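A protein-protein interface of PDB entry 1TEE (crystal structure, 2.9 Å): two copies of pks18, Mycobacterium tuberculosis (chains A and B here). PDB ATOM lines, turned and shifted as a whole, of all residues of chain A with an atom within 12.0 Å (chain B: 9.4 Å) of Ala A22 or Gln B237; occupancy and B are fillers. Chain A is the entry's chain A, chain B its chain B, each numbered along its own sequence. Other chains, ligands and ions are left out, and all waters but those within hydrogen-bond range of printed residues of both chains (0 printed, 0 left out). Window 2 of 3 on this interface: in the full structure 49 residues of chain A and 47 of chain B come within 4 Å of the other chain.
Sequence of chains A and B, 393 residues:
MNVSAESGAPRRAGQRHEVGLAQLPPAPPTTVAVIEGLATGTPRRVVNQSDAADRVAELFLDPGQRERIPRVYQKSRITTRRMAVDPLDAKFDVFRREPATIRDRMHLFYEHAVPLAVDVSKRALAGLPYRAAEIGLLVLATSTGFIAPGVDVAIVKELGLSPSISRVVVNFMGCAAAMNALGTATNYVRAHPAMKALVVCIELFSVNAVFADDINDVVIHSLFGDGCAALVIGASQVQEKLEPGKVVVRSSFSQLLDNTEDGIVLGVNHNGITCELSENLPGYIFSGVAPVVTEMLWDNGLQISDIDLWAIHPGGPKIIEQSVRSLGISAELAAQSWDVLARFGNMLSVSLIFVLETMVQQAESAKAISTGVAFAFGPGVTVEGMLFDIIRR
The side-chain amide oxygen (OE1) of Gln B237 lies close to the backbone carbonyl oxygen (O) of Ala A22, 3.2 Å away. The side-chain amide nitrogen (NE2) of Gln A23 lies within hydrogen-bond range of the side-chain carboxylate (OE2) of Glu B240.
The backbone NH (N) of Val B32 is in hydrogen-bond range of the backbone carbonyl oxygen (O) of Ser B236. The side-chain carboxylate (OE1) of Glu B240 lies within hydrogen-bond range of the side-chain hydroxyl (OG) of Ser B236, at 3.5 Å.
Among the printed residues, pairs that only touch across the chains: Leu A24 with Gln B237 (3.8 Å), Pro A26 with Pro B193 (3.2 Å), Pro A26 with Ser B236 (3.4 Å), Pro A26 with Gln B237 (3.3 Å) and Ala A27 with Pro B193 (3.96 Å).
Of the printed residues of chain B, Gln A23 touches Glu B240 (3.5 Å). Printed residues of chain B within 4 Å of Leu A24: Gln B237. Of the printed residues of chain B, Pro A26 touches Pro B193 (3.2 Å), Ser B236 (3.4 Å) and Gln B237 (3.3 Å). No residue of chain A comes within 4 Å of Val B32. Ala B235 touches none of the printed residues of chain A. Of chain A, only Pro A26 (3.4 Å) comes within 4 Å of Ser B236. Of chain A, only Ala A22 (3.2 Å), Leu A24 (3.8 Å) and Pro A26 (3.3 Å) come within 4 Å of Gln B237. Val B238 touches none of the printed residues of chain A. Glu B240 touches just one residue of chain A: Gln A23 (3.5 Å). The nearest residue of chain B that does not touch Ala A22 is Glu B240 (5.6 Å). The nearest residue of chain A that does not touch Gln B237 is Pro A25 (4.5 Å). The nearest printed residue of chain B that does not touch Leu A24 is Glu B240 (5.5 Å).
Of the 18 printed residues of chain B, 4 touch a printed residue of chain A. Hydrophobic or aromatic side chains of chain B that line the printed part of chain A: Pro B193. Among the printed residues, 7 pairs touch across the chains.
No position is printed for both chains. Of the 7 pairs that touch across the chains among the printed residues, none has its exchanged pair printed and touching as well.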
ATOM      1  N   ALA A  22       1.955  15.827  -2.185  1.00  0.00           N
ATOM      2  CA  ALA A  22       1.598  17.104  -1.496  1.00  0.00           C
ATOM      3  C   ALA A  22       1.764  18.304  -2.438  1.00  0.00           C
ATOM      4  O   ALA A  22       2.720  19.084  -2.317  1.00  0.00           O
ATOM      5  CB  ALA A  22       2.466  17.285  -0.245  1.00  0.00           C
ATOM      6  N   GLN A  23       0.837  18.430  -3.387  1.00  0.00           N
ATOM      7  CA  GLN A  23       0.843  19.536  -4.345  1.00  0.00           C
ATOM      8  C   GLN A  23      -0.256  20.522  -3.956  1.00  0.00           C
ATOM      9  O   GLN A  23      -0.861  21.158  -4.821  1.00  0.00           O
ATOM     10  CB  GLN A  23       0.542  19.056  -5.764  1.00  0.00           C
ATOM     11  CG  GLN A  23       1.539  18.109  -6.382  1.00  0.00           C
ATOM     12  CD  GLN A  23       1.143  17.745  -7.810  1.00  0.00           C
ATOM     13  OE1 GLN A  23       0.021  17.285  -8.058  1.00  0.00           O
ATOM     14  NE2 GLN A  23       2.060  17.952  -8.757  1.00  0.00           N
ATOM     15  N   LEU A  24      -0.539  20.622  -2.661  1.00  0.00           N
ATOM     16  CA  LEU A  24      -1.561  21.547  -2.195  1.00  0.00           C
ATOM     17  C   LEU A  24      -1.084  22.963  -2.465  1.00  0.00           C
ATOM     18  O   LEU A  24       0.111  23.207  -2.618  1.00  0.00           O
ATOM     19  CB  LEU A  24      -1.788  21.394  -0.689  1.00  0.00           C
ATOM     20  CG  LEU A  24      -2.179  20.020  -0.155  1.00  0.00           C
ATOM     21  CD1 LEU A  24      -2.594  20.155   1.316  1.00  0.00           C
ATOM     22  CD2 LEU A  24      -3.318  19.450  -1.000  1.00  0.00           C
ATOM     23  N   PRO A  25      -2.013  23.920  -2.518  1.00  0.00           N
ATOM     24  CA  PRO A  25      -1.610  25.305  -2.769  1.00  0.00           C
ATOM     25  C   PRO A  25      -0.595  25.699  -1.702  1.00  0.00           C
ATOM     26  O   PRO A  25      -0.643  25.199  -0.579  1.00  0.00           O
ATOM     27  CB  PRO A  25      -2.914  26.081  -2.600  1.00  0.00           C
ATOM     28  CG  PRO A  25      -3.982  25.057  -2.877  1.00  0.00           C
ATOM     29  CD  PRO A  25      -3.448  23.834  -2.207  1.00  0.00           C
ATOM     30  N   PRO A  26       0.351  26.577  -2.037  1.00  0.00           N
ATOM     31  CA  PRO A  26       1.322  26.967  -1.012  1.00  0.00           C
ATOM     32  C   PRO A  26       0.607  27.773   0.076  1.00  0.00           C
ATOM     33  O   PRO A  26      -0.422  28.391  -0.181  1.00  0.00           O
ATOM     34  CB  PRO A  26       2.321  27.804  -1.798  1.00  0.00           C
ATOM     35  CG  PRO A  26       2.273  27.173  -3.161  1.00  0.00           C
ATOM     36  CD  PRO A  26       0.802  26.982  -3.378  1.00  0.00           C
ATOM     37  N   ALA A  27       1.135  27.752   1.293  1.00  0.00           N
ATOM     38  CA  ALA A  27       0.516  28.499   2.379  1.00  0.00           C
ATOM     39  C   ALA A  27       0.432  29.958   1.946  1.00  0.00           C
ATOM     40  O   ALA A  27       1.327  30.465   1.274  1.00  0.00           O
ATOM     41  CB  ALA A  27       1.346  28.367   3.649  1.00  0.00           C
ATOM     42  N   PRO A  28      -0.650  30.652   2.319  1.00  0.00           N
ATOM     43  CA  PRO A  28      -0.826  32.056   1.946  1.00  0.00           C
ATOM     44  C   PRO A  28      -0.050  33.023   2.816  1.00  0.00           C
ATOM     45  O   PRO A  28       0.385  32.682   3.920  1.00  0.00           O
ATOM     46  CB  PRO A  28      -2.331  32.281   2.110  1.00  0.00           C
ATOM     47  CG  PRO A  28      -2.911  30.908   2.147  1.00  0.00           C
ATOM     48  CD  PRO A  28      -1.894  30.118   2.887  1.00  0.00           C
ATOM     49  N   PRO A  29       0.143  34.255   2.322  1.00  0.00           N
ATOM     50  CA  PRO A  29       0.868  35.223   3.137  1.00  0.00           C
ATOM     51  C   PRO A  29      -0.055  35.385   4.333  1.00  0.00           C
ATOM     52  O   PRO A  29      -1.242  35.052   4.255  1.00  0.00           O
ATOM     53  CB  PRO A  29       0.906  36.456   2.249  1.00  0.00           C
ATOM     54  CG  PRO A  29       0.912  35.872   0.868  1.00  0.00           C
ATOM     55  CD  PRO A  29      -0.137  34.804   0.985  1.00  0.00           C
ATOM     56  N   THR B  31       7.269  29.921  -2.798  1.00  0.00           N
ATOM     57  CA  THR B  31       6.140  30.104  -3.759  1.00  0.00           C
ATOM     58  C   THR B  31       6.659  30.482  -5.144  1.00  0.00           C
ATOM     59  O   THR B  31       7.624  31.233  -5.271  1.00  0.00           O
ATOM     60  CB  THR B  31       5.178  31.219  -3.305  1.00  0.00           C
ATOM     61  OG1 THR B  31       3.954  31.100  -4.035  1.00  0.00           O
ATOM     62  CG2 THR B  31       5.785  32.617  -3.585  1.00  0.00           C
ATOM     63  N   VAL B  32       6.001  29.982  -6.182  1.00  0.00           N
ATOM     64  CA  VAL B  32       6.434  30.266  -7.541  1.00  0.00           C
ATOM     65  C   VAL B  32       5.279  30.651  -8.434  1.00  0.00           C
ATOM     66  O   VAL B  32       4.204  30.076  -8.342  1.00  0.00           O
ATOM     67  CB  VAL B  32       7.127  29.045  -8.176  1.00  0.00           C
ATOM     68  CG1 VAL B  32       7.663  29.423  -9.524  1.00  0.00           C
ATOM     69  CG2 VAL B  32       8.254  28.547  -7.284  1.00  0.00           C
ATOM     70  N   ALA B  33       5.508  31.624  -9.306  1.00  0.00           N
ATOM     71  CA  ALA B  33       4.478  32.070 -10.241  1.00  0.00           C
ATOM     72  C   ALA B  33       4.623  31.284 -11.552  1.00  0.00           C
ATOM     73  O   ALA B  33       5.681  31.308 -12.184  1.00  0.00           O
ATOM     74  CB  ALA B  33       4.618  33.566 -10.498  1.00  0.00           C
ATOM     75  N   VAL B  34       3.560  30.587 -11.952  1.00  0.00           N
ATOM     76  CA  VAL B  34       3.591  29.786 -13.174  1.00  0.00           C
ATOM     77  C   VAL B  34       2.555  30.150 -14.222  1.00  0.00           C
ATOM     78  O   VAL B  34       1.390  30.392 -13.915  1.00  0.00           O
ATOM     79  CB  VAL B  34       3.407  28.265 -12.870  1.00  0.00           C
ATOM     80  CG1 VAL B  34       3.350  27.478 -14.155  1.00  0.00           C
ATOM     81  CG2 VAL B  34       4.558  27.753 -12.019  1.00  0.00           C
ATOM     82  N   GLU B  36       0.401  28.723 -16.496  1.00  0.00           N
ATOM     83  CA  GLU B  36      -0.152  27.388 -16.692  1.00  0.00           C
ATOM     84  C   GLU B  36      -1.009  27.243 -17.937  1.00  0.00           C
ATOM     85  O   GLU B  36      -1.308  26.135 -18.371  1.00  0.00           O
ATOM     86  CB  GLU B  36      -0.947  26.993 -15.448  1.00  0.00           C
ATOM     87  CG  GLU B  36      -0.127  27.150 -14.182  1.00  0.00           C
ATOM     88  CD  GLU B  36      -0.802  26.587 -12.948  1.00  0.00           C
ATOM     89  OE1 GLU B  36      -2.016  26.848 -12.753  1.00  0.00           O
ATOM     90  OE2 GLU B  36      -0.107  25.897 -12.161  1.00  0.00           O
ATOM     91  N   VAL B 189      -1.845  35.980  -7.362  1.00  0.00           N
ATOM     92  CA  VAL B 189      -1.627  34.558  -7.147  1.00  0.00           C
ATOM     93  C   VAL B 189      -0.664  34.288  -5.990  1.00  0.00           C
ATOM     94  O   VAL B 189      -0.701  33.223  -5.377  1.00  0.00           O
ATOM     95  CB  VAL B 189      -1.098  33.908  -8.452  1.00  0.00           C
ATOM     96  CG1 VAL B 189      -0.021  32.916  -8.152  1.00  0.00           C
ATOM     97  CG2 VAL B 189      -2.235  33.240  -9.194  1.00  0.00           C
ATOM     98  N   PRO B 193      -2.506  31.902  -3.287  1.00  0.00           N
ATOM     99  CA  PRO B 193      -1.986  30.702  -3.950  1.00  0.00           C
ATOM    100  C   PRO B 193      -3.031  29.730  -4.482  1.00  0.00           C
ATOM    101  O   PRO B 193      -2.842  29.119  -5.533  1.00  0.00           O
ATOM    102  CB  PRO B 193      -1.121  30.059  -2.868  1.00  0.00           C
ATOM    103  CG  PRO B 193      -0.676  31.222  -2.054  1.00  0.00           C
ATOM    104  CD  PRO B 193      -1.949  32.018  -1.929  1.00  0.00           C
ATOM    105  N   LYS B 196      -6.351  31.462  -9.108  1.00  0.00           N
ATOM    106  CA  LYS B 196      -5.713  31.559 -10.409  1.00  0.00           C
ATOM    107  C   LYS B 196      -6.044  32.936 -10.961  1.00  0.00           C
ATOM    108  O   LYS B 196      -7.022  33.568 -10.533  1.00  0.00           O
ATOM    109  CB  LYS B 196      -6.253  30.491 -11.350  1.00  0.00           C
ATOM    110  CG  LYS B 196      -6.190  29.097 -10.784  1.00  0.00           C
ATOM    111  CD  LYS B 196      -4.764  28.631 -10.593  1.00  0.00           C
ATOM    112  CE  LYS B 196      -4.740  27.335  -9.806  1.00  0.00           C
ATOM    113  NZ  LYS B 196      -3.456  26.611  -9.961  1.00  0.00           N
ATOM    114  N   GLY B 234      -0.917  30.767 -11.899  1.00  0.00           N
ATOM    115  CA  GLY B 234      -1.195  30.129 -10.626  1.00  0.00           C
ATOM    116  C   GLY B 234       0.056  30.100  -9.758  1.00  0.00           C
ATOM    117  O   GLY B 234       1.174  30.264 -10.259  1.00  0.00           O
ATOM    118  N   ALA B 235      -0.107  29.916  -8.454  1.00  0.00           N
ATOM    119  CA  ALA B 235       1.058  29.858  -7.576  1.00  0.00           C
ATOM    120  C   ALA B 235       1.465  28.400  -7.477  1.00  0.00           C
ATOM    121  O   ALA B 235       0.671  27.521  -7.803  1.00  0.00           O
ATOM    122  CB  ALA B 235       0.715  30.404  -6.205  1.00  0.00           C
ATOM    123  N   SER B 236       2.689  28.128  -7.038  1.00  0.00           N
ATOM    124  CA  SER B 236       3.132  26.746  -6.912  1.00  0.00           C
ATOM    125  C   SER B 236       4.232  26.619  -5.863  1.00  0.00           C
ATOM    126  O   SER B 236       5.036  27.530  -5.692  1.00  0.00           O
ATOM    127  CB  SER B 236       3.615  26.236  -8.267  1.00  0.00           C
ATOM    128  OG  SER B 236       3.649  24.820  -8.294  1.00  0.00           O
ATOM    129  N   GLN B 237       4.257  25.497  -5.150  1.00  0.00           N
ATOM    130  CA  GLN B 237       5.260  25.300  -4.114  1.00  0.00           C
ATOM    131  C   GLN B 237       6.635  25.131  -4.710  1.00  0.00           C
ATOM    132  O   GLN B 237       6.842  24.296  -5.588  1.00  0.00           O
ATOM    133  CB  GLN B 237       4.929  24.086  -3.239  1.00  0.00           C
ATOM    134  CG  GLN B 237       3.706  24.271  -2.334  1.00  0.00           C
ATOM    135  CD  GLN B 237       3.622  23.227  -1.214  1.00  0.00           C
ATOM    136  OE1 GLN B 237       3.624  22.016  -1.468  1.00  0.00           O
ATOM    137  NE2 GLN B 237       3.544  23.701   0.033  1.00  0.00           N
ATOM    138  N   VAL B 238       7.575  25.933  -4.220  1.00  0.00           N
ATOM    139  CA  VAL B 238       8.958  25.908  -4.693  1.00  0.00           C
ATOM    140  C   VAL B 238       9.415  24.489  -5.027  1.00  0.00           C
ATOM    141  O   VAL B 238      10.157  24.277  -5.985  1.00  0.00           O
ATOM    142  CB  VAL B 238       9.929  26.513  -3.635  1.00  0.00           C
ATOM    143  CG1 VAL B 238      11.353  26.474  -4.163  1.00  0.00           C
ATOM    144  CG2 VAL B 238       9.521  27.949  -3.297  1.00  0.00           C
ATOM    145  N   GLN B 239       8.956  23.523  -4.238  1.00  0.00           N
ATOM    146  CA  GLN B 239       9.320  22.126  -4.445  1.00  0.00           C
ATOM    147  C   GLN B 239       8.767  21.582  -5.758  1.00  0.00           C
ATOM    148  O   GLN B 239       9.493  21.483  -6.746  1.00  0.00           O
ATOM    149  CB  GLN B 239       8.816  21.268  -3.273  1.00  0.00           C
ATOM    150  CG  GLN B 239       9.427  21.645  -1.913  1.00  0.00           C
ATOM    151  CD  GLN B 239       8.616  21.127  -0.717  1.00  0.00           C
ATOM    152  OE1 GLN B 239       8.495  19.916  -0.508  1.00  0.00           O
ATOM    153  NE2 GLN B 239       8.056  22.052   0.070  1.00  0.00           N
ATOM    154  N   GLU B 240       7.475  21.252  -5.747  1.00  0.00           N
ATOM    155  CA  GLU B 240       6.750  20.673  -6.888  1.00  0.00           C
ATOM    156  C   GLU B 240       7.428  20.622  -8.264  1.00  0.00           C
ATOM    157  O   GLU B 240       8.047  21.594  -8.707  1.00  0.00           O
ATOM    158  CB  GLU B 240       5.385  21.349  -7.054  1.00  0.00           C
ATOM    159  CG  GLU B 240       4.500  20.592  -8.040  1.00  0.00           C
ATOM    160  CD  GLU B 240       3.163  21.245  -8.272  1.00  0.00           C
ATOM    161  OE1 GLU B 240       2.557  21.705  -7.283  1.00  0.00           O
ATOM    162  OE2 GLU B 240       2.708  21.284  -9.436  1.00  0.00           O
ATOM    163  N   LYS B 241       7.287  19.478  -8.935  1.00  0.00           N
ATOM    164  CA  LYS B 241       7.851  19.276 -10.261  1.00  0.00           C
ATOM    165  C   LYS B 241       6.787  19.565 -11.311  1.00  0.00           C
ATOM    166  O   LYS B 241       5.834  18.811 -11.471  1.00  0.00           O
ATOM    167  CB  LYS B 241       8.353  17.841 -10.405  1.00  0.00           C
ATOM    168  CG  LYS B 241       9.621  17.556  -9.616  1.00  0.00           C
ATOM    169  CD  LYS B 241      10.190  16.185  -9.969  1.00  0.00           C
ATOM    170  CE  LYS B 241      11.532  15.946  -9.282  1.00  0.00           C
ATOM    171  NZ  LYS B 241      12.083  14.574  -9.540  1.00  0.00           N
ATOM    172  N   LEU B 242       6.961  20.662 -12.035  1.00  0.00           N
ATOM    173  CA  LEU B 242       6.004  21.078 -13.053  1.00  0.00           C
ATOM    174  C   LEU B 242       6.104  20.256 -14.335  1.00  0.00           C
ATOM    175  O   LEU B 242       7.179  19.778 -14.693  1.00  0.00           O
ATOM    176  CB  LEU B 242       6.228  22.557 -13.367  1.00  0.00           C
ATOM    177  CG  LEU B 242       6.166  23.464 -12.146  1.00  0.00           C
ATOM    178  CD1 LEU B 242       6.903  24.743 -12.417  1.00  0.00           C
ATOM    179  CD2 LEU B 242       4.726  23.722 -11.791  1.00  0.00           C
ATOM    180  N   VAL B 248       7.838  29.107 -15.728  1.00  0.00           N
ATOM    181  CA  VAL B 248       8.059  29.690 -14.420  1.00  0.00           C
ATOM    182  C   VAL B 248       8.568  31.123 -14.544  1.00  0.00           C
ATOM    183  O   VAL B 248       9.649  31.366 -15.089  1.00  0.00           O
ATOM    184  CB  VAL B 248       9.094  28.869 -13.624  1.00  0.00           C
ATOM    185  CG1 VAL B 248       9.383  29.538 -12.298  1.00  0.00           C
ATOM    186  CG2 VAL B 248       8.581  27.461 -13.412  1.00  0.00           C
